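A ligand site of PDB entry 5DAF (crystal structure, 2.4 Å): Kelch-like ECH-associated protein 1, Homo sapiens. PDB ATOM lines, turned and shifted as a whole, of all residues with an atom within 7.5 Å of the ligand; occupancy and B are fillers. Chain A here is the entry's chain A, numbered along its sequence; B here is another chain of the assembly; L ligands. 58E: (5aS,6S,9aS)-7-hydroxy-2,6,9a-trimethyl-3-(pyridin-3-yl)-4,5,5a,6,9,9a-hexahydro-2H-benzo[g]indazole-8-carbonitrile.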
ATOM      1  N   TYR A  43      -7.339  -2.178  -8.419  1.00  0.00           N
ATOM      2  CA  TYR A  43      -8.176  -1.091  -8.880  1.00  0.00           C
ATOM      3  C   TYR A  43      -8.297  -1.027 -10.406  1.00  0.00           C
ATOM      4  O   TYR A  43      -7.444  -0.443 -11.068  1.00  0.00           O
ATOM      5  CB  TYR A  43      -7.645   0.243  -8.348  1.00  0.00           C
ATOM      6  CG  TYR A  43      -8.352   1.463  -8.906  1.00  0.00           C
ATOM      7  CD1 TYR A  43      -9.503   1.953  -8.300  1.00  0.00           C
ATOM      8  CD2 TYR A  43      -7.858   2.122 -10.028  1.00  0.00           C
ATOM      9  CE1 TYR A  43     -10.160   3.071  -8.804  1.00  0.00           C
ATOM     10  CE2 TYR A  43      -8.504   3.236 -10.540  1.00  0.00           C
ATOM     11  CZ  TYR A  43      -9.651   3.705  -9.922  1.00  0.00           C
ATOM     12  OH  TYR A  43     -10.298   4.820 -10.424  1.00  0.00           O
ATOM     13  N   GLN A  44      -9.333  -1.660 -10.948  1.00  0.00           N
ATOM     14  CA  GLN A  44      -9.929  -1.246 -12.226  1.00  0.00           C
ATOM     15  C   GLN A  44      -8.908  -0.987 -13.371  1.00  0.00           C
ATOM     16  O   GLN A  44      -8.582   0.175 -13.664  1.00  0.00           O
ATOM     17  CB  GLN A  44     -10.742   0.023 -11.942  1.00  0.00           C
ATOM     18  CG  GLN A  44     -11.777   0.448 -12.957  1.00  0.00           C
ATOM     19  CD  GLN A  44     -12.258   1.857 -12.667  1.00  0.00           C
ATOM     20  OE1 GLN A  44     -11.577   2.834 -12.973  1.00  0.00           O
ATOM     21  NE2 GLN A  44     -13.429   1.962 -12.033  1.00  0.00           N
ATOM     22  N   ALA A  46      -5.783  -0.940 -13.681  1.00  0.00           N
ATOM     23  CA  ALA A  46      -4.430  -0.678 -13.168  1.00  0.00           C
ATOM     24  C   ALA A  46      -3.880  -1.942 -12.490  1.00  0.00           C
ATOM     25  O   ALA A  46      -4.645  -2.743 -11.954  1.00  0.00           O
ATOM     26  CB  ALA A  46      -4.441   0.490 -12.198  1.00  0.00           C
ATOM     27  N   GLY A  85     -11.403   0.925  -5.056  1.00  0.00           N
ATOM     28  CA  GLY A  85     -11.872   2.302  -5.228  1.00  0.00           C
ATOM     29  C   GLY A  85     -10.856   3.425  -5.122  1.00  0.00           C
ATOM     30  O   GLY A  85     -11.218   4.594  -5.225  1.00  0.00           O
ATOM     31  N   ILE A  86      -9.588   3.076  -4.915  1.00  0.00           N
ATOM     32  CA  ILE A  86      -8.537   4.076  -4.928  1.00  0.00           C
ATOM     33  C   ILE A  86      -7.369   3.578  -5.754  1.00  0.00           C
ATOM     34  O   ILE A  86      -7.067   2.380  -5.761  1.00  0.00           O
ATOM     35  CB  ILE A  86      -8.123   4.497  -3.492  1.00  0.00           C
ATOM     36  CG1 ILE A  86      -7.142   5.677  -3.527  1.00  0.00           C
ATOM     37  CG2 ILE A  86      -7.585   3.309  -2.709  1.00  0.00           C
ATOM     38  CD1 ILE A  86      -6.813   6.230  -2.153  1.00  0.00           C
ATOM     39  N   HIS A  87      -6.740   4.499  -6.482  1.00  0.00           N
ATOM     40  CA  HIS A  87      -5.602   4.173  -7.332  1.00  0.00           C
ATOM     41  C   HIS A  87      -4.360   3.911  -6.514  1.00  0.00           C
ATOM     42  O   HIS A  87      -4.068   4.650  -5.573  1.00  0.00           O
ATOM     43  CB  HIS A  87      -5.349   5.288  -8.335  1.00  0.00           C
ATOM     44  CG  HIS A  87      -4.360   4.910  -9.410  1.00  0.00           C
ATOM     45  ND1 HIS A  87      -3.082   5.325  -9.395  1.00  0.00           N
ATOM     46  CD2 HIS A  87      -4.499   4.102 -10.536  1.00  0.00           C
ATOM     47  CE1 HIS A  87      -2.432   4.829 -10.469  1.00  0.00           C
ATOM     48  NE2 HIS A  87      -3.313   4.076 -11.161  1.00  0.00           N
ATOM     49  N   PRO A  88      -3.608   2.830  -6.859  1.00  0.00           N
ATOM     50  CA  PRO A  88      -2.383   2.468  -6.130  1.00  0.00           C
ATOM     51  C   PRO A  88      -1.419   3.635  -5.964  1.00  0.00           C
ATOM     52  O   PRO A  88      -0.920   3.857  -4.859  1.00  0.00           O
ATOM     53  CB  PRO A  88      -1.763   1.388  -7.015  1.00  0.00           C
ATOM     54  CG  PRO A  88      -2.926   0.751  -7.669  1.00  0.00           C
ATOM     55  CD  PRO A  88      -3.882   1.869  -7.948  1.00  0.00           C
ATOM     56  N   LYS A  89      -1.194   4.397  -7.024  1.00  0.00           N
ATOM     57  CA  LYS A  89      -0.258   5.517  -6.941  1.00  0.00           C
ATOM     58  C   LYS A  89      -0.734   6.577  -5.950  1.00  0.00           C
ATOM     59  O   LYS A  89       0.078   7.202  -5.272  1.00  0.00           O
ATOM     60  CB  LYS A  89       0.020   6.118  -8.328  1.00  0.00           C
ATOM     61  CG  LYS A  89       1.310   6.939  -8.394  1.00  0.00           C
ATOM     62  CD  LYS A  89       1.814   7.077  -9.831  1.00  0.00           C
ATOM     63  CE  LYS A  89       3.115   7.854  -9.892  1.00  0.00           C
ATOM     64  NZ  LYS A  89       3.528   8.167 -11.292  1.00  0.00           N
ATOM     65  N   VAL A  90      -2.059   6.759  -5.874  1.00  0.00           N
ATOM     66  CA  VAL A  90      -2.669   7.675  -4.898  1.00  0.00           C
ATOM     67  C   VAL A  90      -2.489   7.144  -3.479  1.00  0.00           C
ATOM     68  O   VAL A  90      -2.075   7.885  -2.579  1.00  0.00           O
ATOM     69  CB  VAL A  90      -4.155   7.939  -5.218  1.00  0.00           C
ATOM     70  CG1 VAL A  90      -4.777   8.859  -4.173  1.00  0.00           C
ATOM     71  CG2 VAL A  90      -4.312   8.558  -6.597  1.00  0.00           C
ATOM     72  N   MET A  91      -2.785   5.861  -3.275  1.00  0.00           N
ATOM     73  CA  MET A  91      -2.543   5.231  -1.983  1.00  0.00           C
ATOM     74  C   MET A  91      -1.076   5.374  -1.567  1.00  0.00           C
ATOM     75  O   MET A  91      -0.775   5.785  -0.443  1.00  0.00           O
ATOM     76  CB  MET A  91      -2.954   3.755  -2.022  1.00  0.00           C
ATOM     77  CG  MET A  91      -2.860   3.069  -0.670  1.00  0.00           C
ATOM     78  SD  MET A  91      -4.136   3.586   0.503  1.00  0.00           S
ATOM     79  CE  MET A  91      -3.317   4.861   1.441  1.00  0.00           C
ATOM     80  N   ARG A  93       1.115   7.609  -2.261  1.00  0.00           N
ATOM     81  CA  ARG A  93       1.395   8.988  -1.843  1.00  0.00           C
ATOM     82  C   ARG A  93       0.815   9.339  -0.466  1.00  0.00           C
ATOM     83  O   ARG A  93       1.362  10.200   0.247  1.00  0.00           O
ATOM     84  CB  ARG A  93       0.822   9.975  -2.865  1.00  0.00           C
ATOM     85  CG  ARG A  93       1.443   9.892  -4.250  1.00  0.00           C
ATOM     86  CD  ARG A  93       2.829  10.517  -4.279  1.00  0.00           C
ATOM     87  NE  ARG A  93       3.283  10.667  -5.653  1.00  0.00           N
ATOM     88  CZ  ARG A  93       3.965   9.750  -6.333  1.00  0.00           C
ATOM     89  NH1 ARG A  93       4.279   8.589  -5.772  1.00  0.00           N
ATOM     90  NH2 ARG A  93       4.314   9.988  -7.588  1.00  0.00           N
ATOM     91  N   SER A 104       3.655  14.872  -2.492  1.00  0.00           N
ATOM     92  CA  SER A 104       3.957  15.469  -3.784  1.00  0.00           C
ATOM     93  C   SER A 104       3.193  14.764  -4.896  1.00  0.00           C
ATOM     94  O   SER A 104       3.039  13.548  -4.876  1.00  0.00           O
ATOM     95  CB  SER A 104       5.467  15.395  -4.059  1.00  0.00           C
ATOM     96  OG  SER A 104       5.900  14.052  -4.168  1.00  0.00           O
ATOM     97  N   MET A 105       2.717  15.545  -5.849  1.00  0.00           N
ATOM     98  CA  MET A 105       2.051  15.021  -7.047  1.00  0.00           C
ATOM     99  C   MET A 105       2.182  16.050  -8.178  1.00  0.00           C
ATOM    100  O   MET A 105       2.565  17.208  -7.914  1.00  0.00           O
ATOM    101  CB  MET A 105       0.579  14.666  -6.773  1.00  0.00           C
ATOM    102  CG  MET A 105      -0.328  15.815  -6.346  1.00  0.00           C
ATOM    103  SD  MET A 105       0.115  16.571  -4.771  1.00  0.00           S
ATOM    104  CE  MET A 105      -1.495  16.972  -4.094  1.00  0.00           C
ATOM    105  N   GLY A 106       1.839  15.615  -9.439  1.00  0.00           N
ATOM    106  CA  GLY A 106       2.201  16.519 -10.565  1.00  0.00           C
ATOM    107  C   GLY A 106       1.177  17.515 -11.082  1.00  0.00           C
ATOM    108  O   GLY A 106       1.108  17.737 -12.293  1.00  0.00           O
ATOM    109  N   GLU A 107       0.408  18.127 -10.187  1.00  0.00           N
ATOM    110  CA  GLU A 107      -0.543  19.202 -10.554  1.00  0.00           C
ATOM    111  C   GLU A 107      -1.738  18.692 -11.393  1.00  0.00           C
ATOM    112  O   GLU A 107      -2.892  18.933 -11.028  1.00  0.00           O
ATOM    113  CB  GLU A 107       0.178  20.369 -11.250  1.00  0.00           C
ATOM    114  CG  GLU A 107      -0.702  21.550 -11.642  1.00  0.00           C
ATOM    115  CD  GLU A 107       0.026  22.547 -12.540  1.00  0.00           C
ATOM    116  OE1 GLU A 107      -0.441  22.759 -13.684  1.00  0.00           O
ATOM    117  OE2 GLU A 107       1.057  23.118 -12.107  1.00  0.00           O
ATOM    118  N   LYS A 108      -1.459  18.005 -12.497  1.00  0.00           N
ATOM    119  CA  LYS A 108      -2.491  17.386 -13.334  1.00  0.00           C
ATOM    120  C   LYS A 108      -3.176  16.201 -12.631  1.00  0.00           C
ATOM    121  O   LYS A 108      -3.933  15.451 -13.253  1.00  0.00           O
ATOM    122  CB  LYS A 108      -1.918  16.965 -14.698  1.00  0.00           C
ATOM    123  CG  LYS A 108      -0.915  15.812 -14.673  1.00  0.00           C
ATOM    124  CD  LYS A 108      -0.580  15.322 -16.073  1.00  0.00           C
ATOM    125  CE  LYS A 108       0.324  14.088 -16.060  1.00  0.00           C
ATOM    126  NZ  LYS A 108       1.762  14.408 -15.841  1.00  0.00           N
ATOM    127  N   CYS A 109      -2.910  16.048 -11.331  1.00  0.00           N
ATOM    128  CA  CYS A 109      -3.408  14.913 -10.559  1.00  0.00           C
ATOM    129  C   CYS A 109      -3.723  15.256  -9.107  1.00  0.00           C
ATOM    130  O   CYS A 109      -4.092  14.358  -8.348  1.00  0.00           O
ATOM    131  CB  CYS A 109      -2.383  13.785 -10.562  1.00  0.00           C
ATOM    132  SG  CYS A 109      -2.380  12.856 -12.064  1.00  0.00           S
ATOM    133  N   VAL A 110      -3.570  16.520  -8.704  1.00  0.00           N
ATOM    134  CA  VAL A 110      -3.813  16.907  -7.304  1.00  0.00           C
ATOM    135  C   VAL A 110      -5.268  16.664  -6.861  1.00  0.00           C
ATOM    136  O   VAL A 110      -5.572  16.620  -5.670  1.00  0.00           O
ATOM    137  CB  VAL A 110      -3.386  18.364  -6.968  1.00  0.00           C
ATOM    138  CG1 VAL A 110      -2.084  18.741  -7.667  1.00  0.00           C
ATOM    139  CG2 VAL A 110      -4.475  19.358  -7.303  1.00  0.00           C
ATOM    140  N   HIS A 112      -7.021  13.826  -7.939  1.00  0.00           N
ATOM    141  CA  HIS A 112      -7.052  12.391  -7.663  1.00  0.00           C
ATOM    142  C   HIS A 112      -6.561  12.106  -6.277  1.00  0.00           C
ATOM    143  O   HIS A 112      -7.109  11.249  -5.570  1.00  0.00           O
ATOM    144  CB  HIS A 112      -6.212  11.638  -8.671  1.00  0.00           C
ATOM    145  CG  HIS A 112      -6.814  11.579 -10.046  1.00  0.00           C
ATOM    146  ND1 HIS A 112      -6.276  12.207 -11.108  1.00  0.00           N
ATOM    147  CD2 HIS A 112      -7.967  10.953 -10.506  1.00  0.00           C
ATOM    148  CE1 HIS A 112      -7.029  11.982 -12.194  1.00  0.00           C
ATOM    149  NE2 HIS A 112      -8.070  11.212 -11.826  1.00  0.00           N
ATOM    150  N   VAL A 113      -5.511  12.816  -5.889  1.00  0.00           N
ATOM    151  CA  VAL A 113      -4.929  12.704  -4.559  1.00  0.00           C
ATOM    152  C   VAL A 113      -5.971  13.176  -3.539  1.00  0.00           C
ATOM    153  O   VAL A 113      -6.259  12.489  -2.554  1.00  0.00           O
ATOM    154  CB  VAL A 113      -3.597  13.508  -4.475  1.00  0.00           C
ATOM    155  CG1 VAL A 113      -3.140  13.704  -3.040  1.00  0.00           C
ATOM    156  CG2 VAL A 113      -2.510  12.804  -5.283  1.00  0.00           C
ATOM    157  N   ASN A 115      -9.137  13.253  -3.719  1.00  0.00           N
ATOM    158  CA  ASN A 115     -10.172  12.221  -3.600  1.00  0.00           C
ATOM    159  C   ASN A 115      -9.770  11.055  -2.720  1.00  0.00           C
ATOM    160  O   ASN A 115     -10.598  10.498  -1.993  1.00  0.00           O
ATOM    161  CB  ASN A 115     -10.574  11.705  -4.988  1.00  0.00           C
ATOM    162  CG  ASN A 115     -11.257  12.772  -5.819  1.00  0.00           C
ATOM    163  OD1 ASN A 115     -11.786  13.754  -5.279  1.00  0.00           O
ATOM    164  ND2 ASN A 115     -11.247  12.604  -7.148  1.00  0.00           N
ATOM    165  N   ARG B   8       4.570  20.986 -14.051  1.00  0.00           N
ATOM    166  CA  ARG B   8       4.927  21.359 -12.653  1.00  0.00           C
ATOM    167  C   ARG B   8       4.383  20.330 -11.661  1.00  0.00           C
ATOM    168  O   ARG B   8       3.289  19.798 -11.863  1.00  0.00           O
ATOM    169  CB  ARG B   8       4.395  22.759 -12.319  1.00  0.00           C
ATOM    170  N   THR B   9       5.152  20.048 -10.606  1.00  0.00           N
ATOM    171  CA  THR B   9       4.721  19.108  -9.550  1.00  0.00           C
ATOM    172  C   THR B   9       4.516  19.803  -8.210  1.00  0.00           C
ATOM    173  O   THR B   9       5.459  20.365  -7.639  1.00  0.00           O
ATOM    174  CB  THR B   9       5.699  17.921  -9.365  1.00  0.00           C
ATOM    175  OG1 THR B   9       6.956  18.390  -8.868  1.00  0.00           O
ATOM    176  CG2 THR B   9       5.924  17.161 -10.667  1.00  0.00           C
ATOM    177  N   PHE B  10       3.284  19.766  -7.701  1.00  0.00           N
ATOM    178  CA  PHE B  10       2.919  20.322  -6.401  1.00  0.00           C
ATOM    179  C   PHE B  10       3.507  19.488  -5.264  1.00  0.00           C
ATOM    180  O   PHE B  10       3.656  18.261  -5.386  1.00  0.00           O
ATOM    181  CB  PHE B  10       1.381  20.421  -6.284  1.00  0.00           C
ATOM    182  CG  PHE B  10       0.882  21.029  -4.979  1.00  0.00           C
ATOM    183  CD1 PHE B  10       1.326  22.279  -4.537  1.00  0.00           C
ATOM    184  CD2 PHE B  10      -0.083  20.350  -4.218  1.00  0.00           C
ATOM    185  CE1 PHE B  10       0.845  22.830  -3.347  1.00  0.00           C
ATOM    186  CE2 PHE B  10      -0.572  20.903  -3.039  1.00  0.00           C
ATOM    187  CZ  PHE B  10      -0.100  22.136  -2.602  1.00  0.00           C
HETATM  188  O16 58E L   1       1.588  12.778  -9.478  1.00  0.00           O
HETATM  189  C3  58E L   1       0.612  12.120 -10.100  1.00  0.00           C
HETATM  190  C4  58E L   1       0.016  10.893  -9.421  1.00  0.00           C
HETATM  191  C17 58E L   1      -0.274  11.220  -7.954  1.00  0.00           C
HETATM  192  C5  58E L   1      -1.239  10.359 -10.127  1.00  0.00           C
HETATM  193  C6  58E L   1      -1.725   9.012  -9.575  1.00  0.00           C
HETATM  194  C7  58E L   1      -3.169   8.670  -9.967  1.00  0.00           C
HETATM  195  C8  58E L   1      -3.346   8.994 -11.435  1.00  0.00           C
HETATM  196  C13 58E L   1      -4.397   8.665 -12.442  1.00  0.00           C
HETATM  197  C20 58E L   1      -5.649   7.867 -12.270  1.00  0.00           C
HETATM  198  C25 58E L   1      -6.057   6.960 -13.242  1.00  0.00           C
HETATM  199  C24 58E L   1      -7.231   6.237 -13.061  1.00  0.00           C
HETATM  200  C23 58E L   1      -7.990   6.451 -11.909  1.00  0.00           C
HETATM  201  N22 58E L   1      -7.578   7.336 -10.986  1.00  0.00           N
HETATM  202  C21 58E L   1      -6.443   8.048 -11.142  1.00  0.00           C
HETATM  203  N12 58E L   1      -3.966   9.255 -13.591  1.00  0.00           N
HETATM  204  C19 58E L   1      -4.537   9.332 -14.968  1.00  0.00           C
HETATM  205  N11 58E L   1      -2.750   9.942 -13.469  1.00  0.00           N
HETATM  206  C9  58E L   1      -2.376   9.796 -12.181  1.00  0.00           C
HETATM  207  C10 58E L   1      -1.104  10.394 -11.669  1.00  0.00           C
HETATM  208  C18 58E L   1       0.039   9.518 -12.194  1.00  0.00           C
HETATM  209  C1  58E L   1      -0.903  11.860 -12.102  1.00  0.00           C
HETATM  210  C2  58E L   1       0.196  12.544 -11.318  1.00  0.00           C
HETATM  211  C14 58E L   1       0.728  13.563 -11.844  1.00  0.00           C
HETATM  212  N15 58E L   1       1.191  14.441 -12.455  1.00  0.00           N
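A nitrogen (N15) of the ligand lies close to the side-chain amino group of Lys 108, at 3.4 Å. The backbone NH of Gly 106 sits at hydrogen-bond distance from an oxygen (O16) of the ligand (2.8 Å). A carbon (C1) of the ligand is bonded to the side-chain sulfur of Cys 109 (1.8 Å).
The backbone NH (N) of Lys 89 is in hydrogen-bond range of a ring nitrogen (ND1) of His 87. The backbone carbonyl oxygen (O) of Met 105 is in hydrogen-bond range of the backbone NH (N) of Phe 10 of chain B (2.7 Å). The side-chain hydroxyl (OH) of Tyr 43 sits at hydrogen-bond distance from the side-chain amide oxygen (OE1) of Gln 44, 3.5 Å away.
Residues that only touch the ligand: Tyr 43 (3.2 Å), Met 105 (3.3 Å), His 112 (3.3 Å), His 87 (3.4 Å), Val 90 (3.6 Å), Lys 89 (3.6 Å) and Val 113 (3.8 Å). Hydrophobic or aromatic side chains within 4 Å of the ligand: Tyr 43, His 87, Val 90, Met 105, His 112 and Val 113. Within 4 Å of the ligand: Tyr 43, His 87, Lys 89, Val 90, Met 105, Gly 106, Lys 108, Cys 109, His 112 and Val 113.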
